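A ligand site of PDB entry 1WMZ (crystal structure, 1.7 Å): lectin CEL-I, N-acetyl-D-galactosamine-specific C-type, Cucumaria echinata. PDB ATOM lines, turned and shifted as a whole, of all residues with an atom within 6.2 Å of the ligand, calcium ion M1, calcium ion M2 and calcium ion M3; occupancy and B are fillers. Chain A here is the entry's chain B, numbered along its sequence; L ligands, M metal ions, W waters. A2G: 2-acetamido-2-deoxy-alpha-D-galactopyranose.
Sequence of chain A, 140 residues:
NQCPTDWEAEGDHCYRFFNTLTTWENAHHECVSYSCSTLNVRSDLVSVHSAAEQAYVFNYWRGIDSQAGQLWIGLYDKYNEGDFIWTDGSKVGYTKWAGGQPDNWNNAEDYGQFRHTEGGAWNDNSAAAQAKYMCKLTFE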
ATOM      1  N   GLN A  70      20.934 -23.138  -9.772  1.00  0.00           N
ATOM      2  CA  GLN A  70      21.446 -23.753 -10.982  1.00  0.00           C
ATOM      3  C   GLN A  70      22.955 -23.881 -10.937  1.00  0.00           C
ATOM      4  O   GLN A  70      23.632 -23.250 -10.134  1.00  0.00           O
ATOM      5  CB  GLN A  70      20.958 -22.980 -12.217  1.00  0.00           C
ATOM      6  CG  GLN A  70      19.422 -23.064 -12.444  1.00  0.00           C
ATOM      7  CD  GLN A  70      18.659 -22.083 -11.582  1.00  0.00           C
ATOM      8  OE1 GLN A  70      19.012 -20.885 -11.537  1.00  0.00           O
ATOM      9  NE2 GLN A  70      17.615 -22.581 -10.867  1.00  0.00           N
ATOM     10  N   ASP A  77      25.276 -20.941 -26.964  1.00  0.00           N
ATOM     11  CA  ASP A  77      24.956 -20.639 -28.369  1.00  0.00           C
ATOM     12  C   ASP A  77      25.171 -19.178 -28.703  1.00  0.00           C
ATOM     13  O   ASP A  77      24.607 -18.681 -29.683  1.00  0.00           O
ATOM     14  CB  ASP A  77      23.549 -21.086 -28.818  1.00  0.00           C
ATOM     15  CG  ASP A  77      22.436 -20.238 -28.259  1.00  0.00           C
ATOM     16  OD1 ASP A  77      22.669 -19.496 -27.260  1.00  0.00           O
ATOM     17  OD2 ASP A  77      21.262 -20.249 -28.773  1.00  0.00           O
ATOM     18  N   LYS A  78      26.044 -18.530 -27.924  1.00  0.00           N
ATOM     19  CA  LYS A  78      26.421 -17.142 -28.076  1.00  0.00           C
ATOM     20  C   LYS A  78      26.805 -16.732 -29.492  1.00  0.00           C
ATOM     21  O   LYS A  78      26.420 -15.642 -29.927  1.00  0.00           O
ATOM     22  CB  LYS A  78      27.560 -16.806 -27.093  1.00  0.00           C
ATOM     23  CG  LYS A  78      28.242 -15.474 -27.195  1.00  0.00           C
ATOM     24  CD  LYS A  78      29.429 -15.407 -26.174  1.00  0.00           C
ATOM     25  CE  LYS A  78      29.986 -14.010 -26.115  1.00  0.00           C
ATOM     26  NZ  LYS A  78      30.977 -13.905 -24.997  1.00  0.00           N
ATOM     27  N   GLU A  81      23.078 -18.640 -32.766  1.00  0.00           N
ATOM     28  CA  GLU A  81      21.842 -18.814 -32.012  1.00  0.00           C
ATOM     29  C   GLU A  81      21.159 -20.088 -32.414  1.00  0.00           C
ATOM     30  O   GLU A  81      20.947 -20.362 -33.610  1.00  0.00           O
ATOM     31  CB  GLU A  81      20.921 -17.607 -32.243  1.00  0.00           C
ATOM     32  CG  GLU A  81      19.549 -17.720 -31.581  1.00  0.00           C
ATOM     33  CD  GLU A  81      19.662 -17.857 -30.065  1.00  0.00           C
ATOM     34  OE1 GLU A  81      18.887 -18.637 -29.488  1.00  0.00           O
ATOM     35  OE2 GLU A  81      20.505 -17.157 -29.472  1.00  0.00           O
ATOM     36  N   GLY A  82      20.804 -20.886 -31.419  1.00  0.00           N
ATOM     37  CA  GLY A  82      20.061 -22.085 -31.619  1.00  0.00           C
ATOM     38  C   GLY A  82      20.921 -23.320 -31.784  1.00  0.00           C
ATOM     39  O   GLY A  82      20.360 -24.440 -31.715  1.00  0.00           O
ATOM     40  N   PHE A  84      23.608 -25.047 -29.786  1.00  0.00           N
ATOM     41  CA  PHE A  84      24.424 -25.171 -28.552  1.00  0.00           C
ATOM     42  C   PHE A  84      25.658 -26.061 -28.729  1.00  0.00           C
ATOM     43  O   PHE A  84      25.555 -27.178 -29.249  1.00  0.00           O
ATOM     44  CB  PHE A  84      23.577 -25.624 -27.345  1.00  0.00           C
ATOM     45  CG  PHE A  84      22.726 -24.544 -26.816  1.00  0.00           C
ATOM     46  CD1 PHE A  84      23.181 -23.733 -25.802  1.00  0.00           C
ATOM     47  CD2 PHE A  84      21.484 -24.264 -27.376  1.00  0.00           C
ATOM     48  CE1 PHE A  84      22.427 -22.683 -25.312  1.00  0.00           C
ATOM     49  CE2 PHE A  84      20.733 -23.176 -26.902  1.00  0.00           C
ATOM     50  CZ  PHE A  84      21.206 -22.396 -25.874  1.00  0.00           C
ATOM     51  N   GLY A 100      10.479 -27.891 -22.269  1.00  0.00           N
ATOM     52  CA  GLY A 100      10.313 -26.503 -22.637  1.00  0.00           C
ATOM     53  C   GLY A 100      11.569 -25.725 -22.928  1.00  0.00           C
ATOM     54  O   GLY A 100      11.510 -24.565 -23.359  1.00  0.00           O
ATOM     55  N   GLN A 101      12.717 -26.353 -22.710  1.00  0.00           N
ATOM     56  CA  GLN A 101      14.003 -25.731 -22.951  1.00  0.00           C
ATOM     57  C   GLN A 101      14.774 -26.428 -24.086  1.00  0.00           C
ATOM     58  O   GLN A 101      14.485 -27.613 -24.400  1.00  0.00           O
ATOM     59  CB  GLN A 101      14.834 -25.775 -21.676  1.00  0.00           C
ATOM     60  CG  GLN A 101      14.117 -25.183 -20.451  1.00  0.00           C
ATOM     61  CD  GLN A 101      13.777 -23.730 -20.601  1.00  0.00           C
ATOM     62  OE1 GLN A 101      14.470 -22.999 -21.306  1.00  0.00           O
ATOM     63  NE2 GLN A 101      12.706 -23.283 -19.914  1.00  0.00           N
ATOM     64  N   PRO A 102      15.710 -25.733 -24.728  1.00  0.00           N
ATOM     65  CA  PRO A 102      16.003 -24.325 -24.536  1.00  0.00           C
ATOM     66  C   PRO A 102      14.938 -23.464 -25.181  1.00  0.00           C
ATOM     67  O   PRO A 102      14.385 -23.864 -26.223  1.00  0.00           O
ATOM     68  CB  PRO A 102      17.338 -24.152 -25.275  1.00  0.00           C
ATOM     69  CG  PRO A 102      17.272 -25.211 -26.411  1.00  0.00           C
ATOM     70  CD  PRO A 102      16.430 -26.288 -25.904  1.00  0.00           C
ATOM     71  N   ASP A 103      14.717 -22.264 -24.644  1.00  0.00           N
ATOM     72  CA  ASP A 103      13.720 -21.371 -25.202  1.00  0.00           C
ATOM     73  C   ASP A 103      14.210 -19.963 -25.621  1.00  0.00           C
ATOM     74  O   ASP A 103      13.429 -19.182 -26.151  1.00  0.00           O
ATOM     75  CB  ASP A 103      12.555 -21.282 -24.222  1.00  0.00           C
ATOM     76  CG  ASP A 103      12.940 -20.659 -22.918  1.00  0.00           C
ATOM     77  OD1 ASP A 103      12.061 -20.370 -22.054  1.00  0.00           O
ATOM     78  OD2 ASP A 103      14.128 -20.387 -22.708  1.00  0.00           O
ATOM     79  N   ASN A 104      15.488 -19.685 -25.467  1.00  0.00           N
ATOM     80  CA  ASN A 104      16.057 -18.392 -25.824  1.00  0.00           C
ATOM     81  C   ASN A 104      15.220 -17.232 -25.304  1.00  0.00           C
ATOM     82  O   ASN A 104      14.819 -16.338 -26.047  1.00  0.00           O
ATOM     83  CB  ASN A 104      16.221 -18.245 -27.360  1.00  0.00           C
ATOM     84  CG  ASN A 104      17.226 -17.120 -27.740  1.00  0.00           C
ATOM     85  OD1 ASN A 104      18.272 -16.912 -27.091  1.00  0.00           O
ATOM     86  ND2 ASN A 104      16.884 -16.383 -28.812  1.00  0.00           N
ATOM     87  N   TRP A 105      14.888 -17.294 -24.037  1.00  0.00           N
ATOM     88  CA  TRP A 105      13.878 -16.388 -23.483  1.00  0.00           C
ATOM     89  C   TRP A 105      14.264 -14.923 -23.681  1.00  0.00           C
ATOM     90  O   TRP A 105      15.387 -14.521 -23.428  1.00  0.00           O
ATOM     91  CB  TRP A 105      13.589 -16.691 -22.009  1.00  0.00           C
ATOM     92  CG  TRP A 105      12.368 -15.938 -21.480  1.00  0.00           C
ATOM     93  CD1 TRP A 105      12.374 -14.867 -20.606  1.00  0.00           C
ATOM     94  CD2 TRP A 105      10.989 -16.157 -21.823  1.00  0.00           C
ATOM     95  NE1 TRP A 105      11.085 -14.415 -20.400  1.00  0.00           N
ATOM     96  CE2 TRP A 105      10.215 -15.210 -21.089  1.00  0.00           C
ATOM     97  CE3 TRP A 105      10.313 -17.089 -22.606  1.00  0.00           C
ATOM     98  CZ2 TRP A 105       8.801 -15.156 -21.164  1.00  0.00           C
ATOM     99  CZ3 TRP A 105       8.888 -17.043 -22.677  1.00  0.00           C
ATOM    100  CH2 TRP A 105       8.158 -16.079 -21.963  1.00  0.00           C
ATOM    101  N   ASN A 107      14.975 -13.395 -26.259  1.00  0.00           N
ATOM    102  CA  ASN A 107      16.094 -13.376 -27.189  1.00  0.00           C
ATOM    103  C   ASN A 107      17.457 -13.145 -26.551  1.00  0.00           C
ATOM    104  O   ASN A 107      18.356 -12.596 -27.174  1.00  0.00           O
ATOM    105  CB  ASN A 107      15.855 -12.328 -28.298  1.00  0.00           C
ATOM    106  CG  ASN A 107      16.639 -12.641 -29.526  1.00  0.00           C
ATOM    107  OD1 ASN A 107      16.627 -13.773 -29.984  1.00  0.00           O
ATOM    108  ND2 ASN A 107      17.354 -11.638 -30.070  1.00  0.00           N
ATOM    109  N   ALA A 108      17.627 -13.604 -25.312  1.00  0.00           N
ATOM    110  CA  ALA A 108      18.771 -13.254 -24.493  1.00  0.00           C
ATOM    111  C   ALA A 108      19.393 -14.431 -23.714  1.00  0.00           C
ATOM    112  O   ALA A 108      20.337 -14.233 -22.931  1.00  0.00           O
ATOM    113  CB  ALA A 108      18.379 -12.102 -23.520  1.00  0.00           C
ATOM    114  N   GLU A 109      18.986 -15.663 -23.995  1.00  0.00           N
ATOM    115  CA  GLU A 109      19.491 -16.816 -23.239  1.00  0.00           C
ATOM    116  C   GLU A 109      20.394 -17.658 -24.076  1.00  0.00           C
ATOM    117  O   GLU A 109      19.914 -18.340 -24.976  1.00  0.00           O
ATOM    118  CB  GLU A 109      18.333 -17.635 -22.685  1.00  0.00           C
ATOM    119  CG  GLU A 109      17.541 -16.818 -21.660  1.00  0.00           C
ATOM    120  CD  GLU A 109      16.606 -17.662 -20.850  1.00  0.00           C
ATOM    121  OE1 GLU A 109      16.033 -18.597 -21.451  1.00  0.00           O
ATOM    122  OE2 GLU A 109      16.416 -17.422 -19.608  1.00  0.00           O
ATOM    123  N   ASP A 110      21.687 -17.596 -23.789  1.00  0.00           N
ATOM    124  CA  ASP A 110      22.707 -18.329 -24.578  1.00  0.00           C
ATOM    125  C   ASP A 110      23.645 -19.211 -23.769  1.00  0.00           C
ATOM    126  O   ASP A 110      24.603 -19.738 -24.333  1.00  0.00           O
ATOM    127  CB  ASP A 110      23.565 -17.335 -25.389  1.00  0.00           C
ATOM    128  CG  ASP A 110      22.735 -16.350 -26.226  1.00  0.00           C
ATOM    129  OD1 ASP A 110      21.626 -16.625 -26.742  1.00  0.00           O
ATOM    130  OD2 ASP A 110      23.147 -15.203 -26.439  1.00  0.00           O
ATOM    131  N   TYR A 111      23.357 -19.432 -22.486  1.00  0.00           N
ATOM    132  CA  TYR A 111      24.312 -20.079 -21.565  1.00  0.00           C
ATOM    133  C   TYR A 111      23.627 -21.199 -20.836  1.00  0.00           C
ATOM    134  O   TYR A 111      22.598 -21.017 -20.191  1.00  0.00           O
ATOM    135  CB  TYR A 111      24.883 -19.012 -20.607  1.00  0.00           C
ATOM    136  CG  TYR A 111      25.401 -17.824 -21.426  1.00  0.00           C
ATOM    137  CD1 TYR A 111      24.674 -16.640 -21.535  1.00  0.00           C
ATOM    138  CD2 TYR A 111      26.522 -17.975 -22.197  1.00  0.00           C
ATOM    139  CE1 TYR A 111      25.134 -15.570 -22.320  1.00  0.00           C
ATOM    140  CE2 TYR A 111      26.984 -16.945 -23.002  1.00  0.00           C
ATOM    141  CZ  TYR A 111      26.289 -15.740 -23.059  1.00  0.00           C
ATOM    142  OH  TYR A 111      26.756 -14.734 -23.895  1.00  0.00           O
ATOM    143  N   GLN A 113      23.028 -24.399 -18.225  1.00  0.00           N
ATOM    144  CA  GLN A 113      23.141 -24.718 -16.796  1.00  0.00           C
ATOM    145  C   GLN A 113      22.234 -25.915 -16.409  1.00  0.00           C
ATOM    146  O   GLN A 113      21.214 -26.105 -17.030  1.00  0.00           O
ATOM    147  CB  GLN A 113      22.752 -23.485 -15.964  1.00  0.00           C
ATOM    148  CG  GLN A 113      21.336 -23.035 -16.234  1.00  0.00           C
ATOM    149  CD  GLN A 113      20.824 -21.800 -15.522  1.00  0.00           C
ATOM    150  OE1 GLN A 113      19.600 -21.596 -15.497  1.00  0.00           O
ATOM    151  NE2 GLN A 113      21.711 -20.956 -14.998  1.00  0.00           N
ATOM    152  N   ARG A 115      19.543 -27.438 -13.859  1.00  0.00           N
ATOM    153  CA  ARG A 115      18.669 -27.185 -12.711  1.00  0.00           C
ATOM    154  C   ARG A 115      19.032 -28.128 -11.539  1.00  0.00           C
ATOM    155  O   ARG A 115      19.698 -29.180 -11.734  1.00  0.00           O
ATOM    156  CB  ARG A 115      17.214 -27.373 -13.076  1.00  0.00           C
ATOM    157  CG  ARG A 115      16.682 -26.423 -14.137  1.00  0.00           C
ATOM    158  CD  ARG A 115      15.281 -26.754 -14.548  1.00  0.00           C
ATOM    159  NE  ARG A 115      14.673 -25.700 -15.369  1.00  0.00           N
ATOM    160  CZ  ARG A 115      13.504 -25.811 -15.996  1.00  0.00           C
ATOM    161  NH1 ARG A 115      12.796 -26.950 -15.895  1.00  0.00           N
ATOM    162  NH2 ARG A 115      13.029 -24.787 -16.699  1.00  0.00           N
ATOM    163  N   ASN A 123      18.833 -25.999 -18.675  1.00  0.00           N
ATOM    164  CA  ASN A 123      18.164 -24.777 -19.088  1.00  0.00           C
ATOM    165  C   ASN A 123      19.189 -23.830 -19.748  1.00  0.00           C
ATOM    166  O   ASN A 123      20.343 -23.822 -19.425  1.00  0.00           O
ATOM    167  CB  ASN A 123      17.577 -24.053 -17.833  1.00  0.00           C
ATOM    168  CG  ASN A 123      17.014 -22.694 -18.196  1.00  0.00           C
ATOM    169  OD1 ASN A 123      16.197 -22.599 -19.101  1.00  0.00           O
ATOM    170  ND2 ASN A 123      17.445 -21.635 -17.508  1.00  0.00           N
ATOM    171  N   ASP A 124      18.717 -23.031 -20.695  1.00  0.00           N
ATOM    172  CA  ASP A 124      19.460 -21.882 -21.208  1.00  0.00           C
ATOM    173  C   ASP A 124      19.063 -20.646 -20.392  1.00  0.00           C
ATOM    174  O   ASP A 124      17.864 -20.378 -20.195  1.00  0.00           O
ATOM    175  CB  ASP A 124      19.266 -21.660 -22.712  1.00  0.00           C
ATOM    176  CG  ASP A 124      17.874 -21.402 -23.162  1.00  0.00           C
ATOM    177  OD1 ASP A 124      16.847 -21.788 -22.481  1.00  0.00           O
ATOM    178  OD2 ASP A 124      17.729 -20.864 -24.293  1.00  0.00           O
ATOM    179  N   ASN A 125      20.050 -19.878 -19.998  1.00  0.00           N
ATOM    180  CA  ASN A 125      19.800 -18.630 -19.272  1.00  0.00           C
ATOM    181  C   ASN A 125      20.660 -17.484 -19.817  1.00  0.00           C
ATOM    182  O   ASN A 125      21.414 -17.662 -20.773  1.00  0.00           O
ATOM    183  CB  ASN A 125      20.066 -18.894 -17.776  1.00  0.00           C
ATOM    184  CG  ASN A 125      19.089 -18.174 -16.880  1.00  0.00           C
ATOM    185  OD1 ASN A 125      18.732 -17.019 -17.157  1.00  0.00           O
ATOM    186  ND2 ASN A 125      18.651 -18.855 -15.796  1.00  0.00           N
ATOM    187  N   SER A 126      20.471 -16.304 -19.234  1.00  0.00           N
ATOM    188  CA  SER A 126      21.003 -15.063 -19.747  1.00  0.00           C
ATOM    189  C   SER A 126      22.364 -14.720 -19.147  1.00  0.00           C
ATOM    190  O   SER A 126      22.866 -15.365 -18.239  1.00  0.00           O
ATOM    191  CB  SER A 126      20.039 -13.930 -19.453  1.00  0.00           C
ATOM    192  OG  SER A 126      20.109 -13.703 -18.063  1.00  0.00           O
HETATM  193  O5  A2G L   1      11.559 -20.201 -17.428  1.00  0.00           O
HETATM  194  C1  A2G L   1      12.529 -20.605 -16.502  1.00  0.00           C
HETATM  195  O1  A2G L   1      12.509 -19.440 -15.641  1.00  0.00           O
HETATM  196  C2  A2G L   1      13.980 -20.584 -16.902  1.00  0.00           C
HETATM  197  N2  A2G L   1      14.888 -20.627 -15.795  1.00  0.00           N
HETATM  198  C3  A2G L   1      14.353 -19.506 -17.910  1.00  0.00           C
HETATM  199  O3  A2G L   1      15.561 -19.683 -18.598  1.00  0.00           O
HETATM  200  C4  A2G L   1      13.244 -19.121 -18.854  1.00  0.00           C
HETATM  201  O4  A2G L   1      13.248 -20.247 -19.799  1.00  0.00           O
HETATM  202  C5  A2G L   1      11.819 -19.176 -18.360  1.00  0.00           C
HETATM  203  C6  A2G L   1      10.703 -19.117 -19.368  1.00  0.00           C
HETATM  204  O6  A2G L   1       9.447 -18.741 -18.676  1.00  0.00           O
HETATM  205  C7  A2G L   1      15.323 -21.795 -15.305  1.00  0.00           C
HETATM  206  O7  A2G L   1      15.052 -22.873 -15.790  1.00  0.00           O
HETATM  207  C8  A2G L   1      16.189 -21.686 -14.106  1.00  0.00           C
HETATM  208 CA    CA M   1      20.215 -18.518 -27.427  1.00  0.00          CA
HETATM  209 CA    CA M   2      15.593 -20.881 -20.761  1.00  0.00          CA
HETATM  210 CA    CA M   3      21.809 -15.177 -28.743  1.00  0.00          CA
HETATM  211  O   HOH W   1      23.232 -16.206 -30.011  1.00  0.00           O
HETATM  212  O   HOH W   2      20.337 -14.465 -30.619  1.00  0.00           O
HETATM  213  O   HOH W   3       8.749 -18.628 -16.218  1.00  0.00           O
HETATM  214  O   HOH W   4      15.741 -18.004 -14.240  1.00  0.00           O
HETATM  215  O   HOH W   5      18.826 -20.272 -26.748  1.00  0.00           O
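Calcium ion M2 is bound by OD1 of Asp 124, O of Asp 124, OE1 of Glu 109, OE1 of Gln 101, OD1 of Asn 123, O3 of the ligand, OD2 of Asp 103 and O4 of the ligand.
Calcium ion M2 has eight donor atoms within binding distance.
Of the 23 residues printed, 5 come within 4 Å of calcium ion M2.
The side-chain amide nitrogen of Asn 123 lies close to the side-chain amide nitrogen of Asn 125 (3.5 Å).
The side-chain carboxylate (OD2) of Asp 77 lies close to the backbone NH (N) of Gly 82, 2.8 Å away.
OD1 of Asn 107 sits at hydrogen-bond distance from ND2 of Asn 104 (2.9 Å).
The backbone NH (N) of Trp 105 lies close to the side-chain carboxylate (OE1) of Glu 109, 3.1 Å away.
OE1 of Gln 113 sits at hydrogen-bond distance from ND2 of Asn 125 (2.9 Å).
The backbone NH (N) of Asn 123 sits at hydrogen-bond distance from the backbone carbonyl oxygen (O) of Gln 113 (2.9 Å).
The backbone NH (N) of Asn 104 is in hydrogen-bond range of the side-chain carboxylate (OD2) of Asp 124 (2.8 Å).
The backbone NH (N) of Asp 110 lies within hydrogen-bond range of the backbone carbonyl oxygen (O) of Asn 125 (3.0 Å).
Water W4 bridges N2 of the ligand (3.2 Å) and ND2 of Asn 125 (3.4 Å).
Within 4 Å of calcium ion M3: Glu 81 and Asp 110.
The nearest printed residue that does not touch calcium ion M3 is Asn 104 (4.3 Å).
Gln 70 touches the ligand.
CE3 of Trp 105 touches C6 of the ligand, at 3.8 Å.
OE1 of Gln 113 touches C8 of the ligand, at 3.7 Å.
Hydrophobic or aromatic side chains that line the ligand: Trp 105.
Nine residues have an atom within 4 Å of the ligand: Gln 70, Gln 101, Asp 103, Trp 105, Glu 109, Gln 113, Arg 115, Asn 123 and Asp 124.
Along chain A the residues within 4 Å of the ligand span positions 70 to 124.
The nearest printed residue that does not touch the ligand is Asn 125 (4.1 Å).
O7 of the ligand is in hydrogen-bond range of NE of Arg 115 (2.9 Å).
Calcium ion M3 is bound by water W1 (2.2 Å), the side-chain carboxylate (OD1) of Asp 110 (2.5 Å), the side-chain carboxylate (OE2) of Glu 81 (2.5 Å), water W2 (2.5 Å) and the side-chain carboxylate (OD2) of Asp 110 (2.7 Å).
Calcium ion M1 is bound by water W5 (2.3 Å).
OD2 of Asp 77 binds calcium ion M1.
OE1 of Glu 81 binds calcium ion M1, at 2.5 Å.
Calcium ion M1 is bound by OD1 of Asp 110, at 2.5 Å.
Calcium ion M1 is bound by OE2 of Glu 81 (2.5 Å).
Calcium ion M1 is bound by the backbone carbonyl oxygen (O) of Glu 109 (2.5 Å).
OD1 of Asn 104 binds calcium ion M1 (2.5 Å).
OD1 of Asp 77 is bound to calcium ion M1 (2.6 Å).
Calcium ion M1 has eight donor atoms within binding distance.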
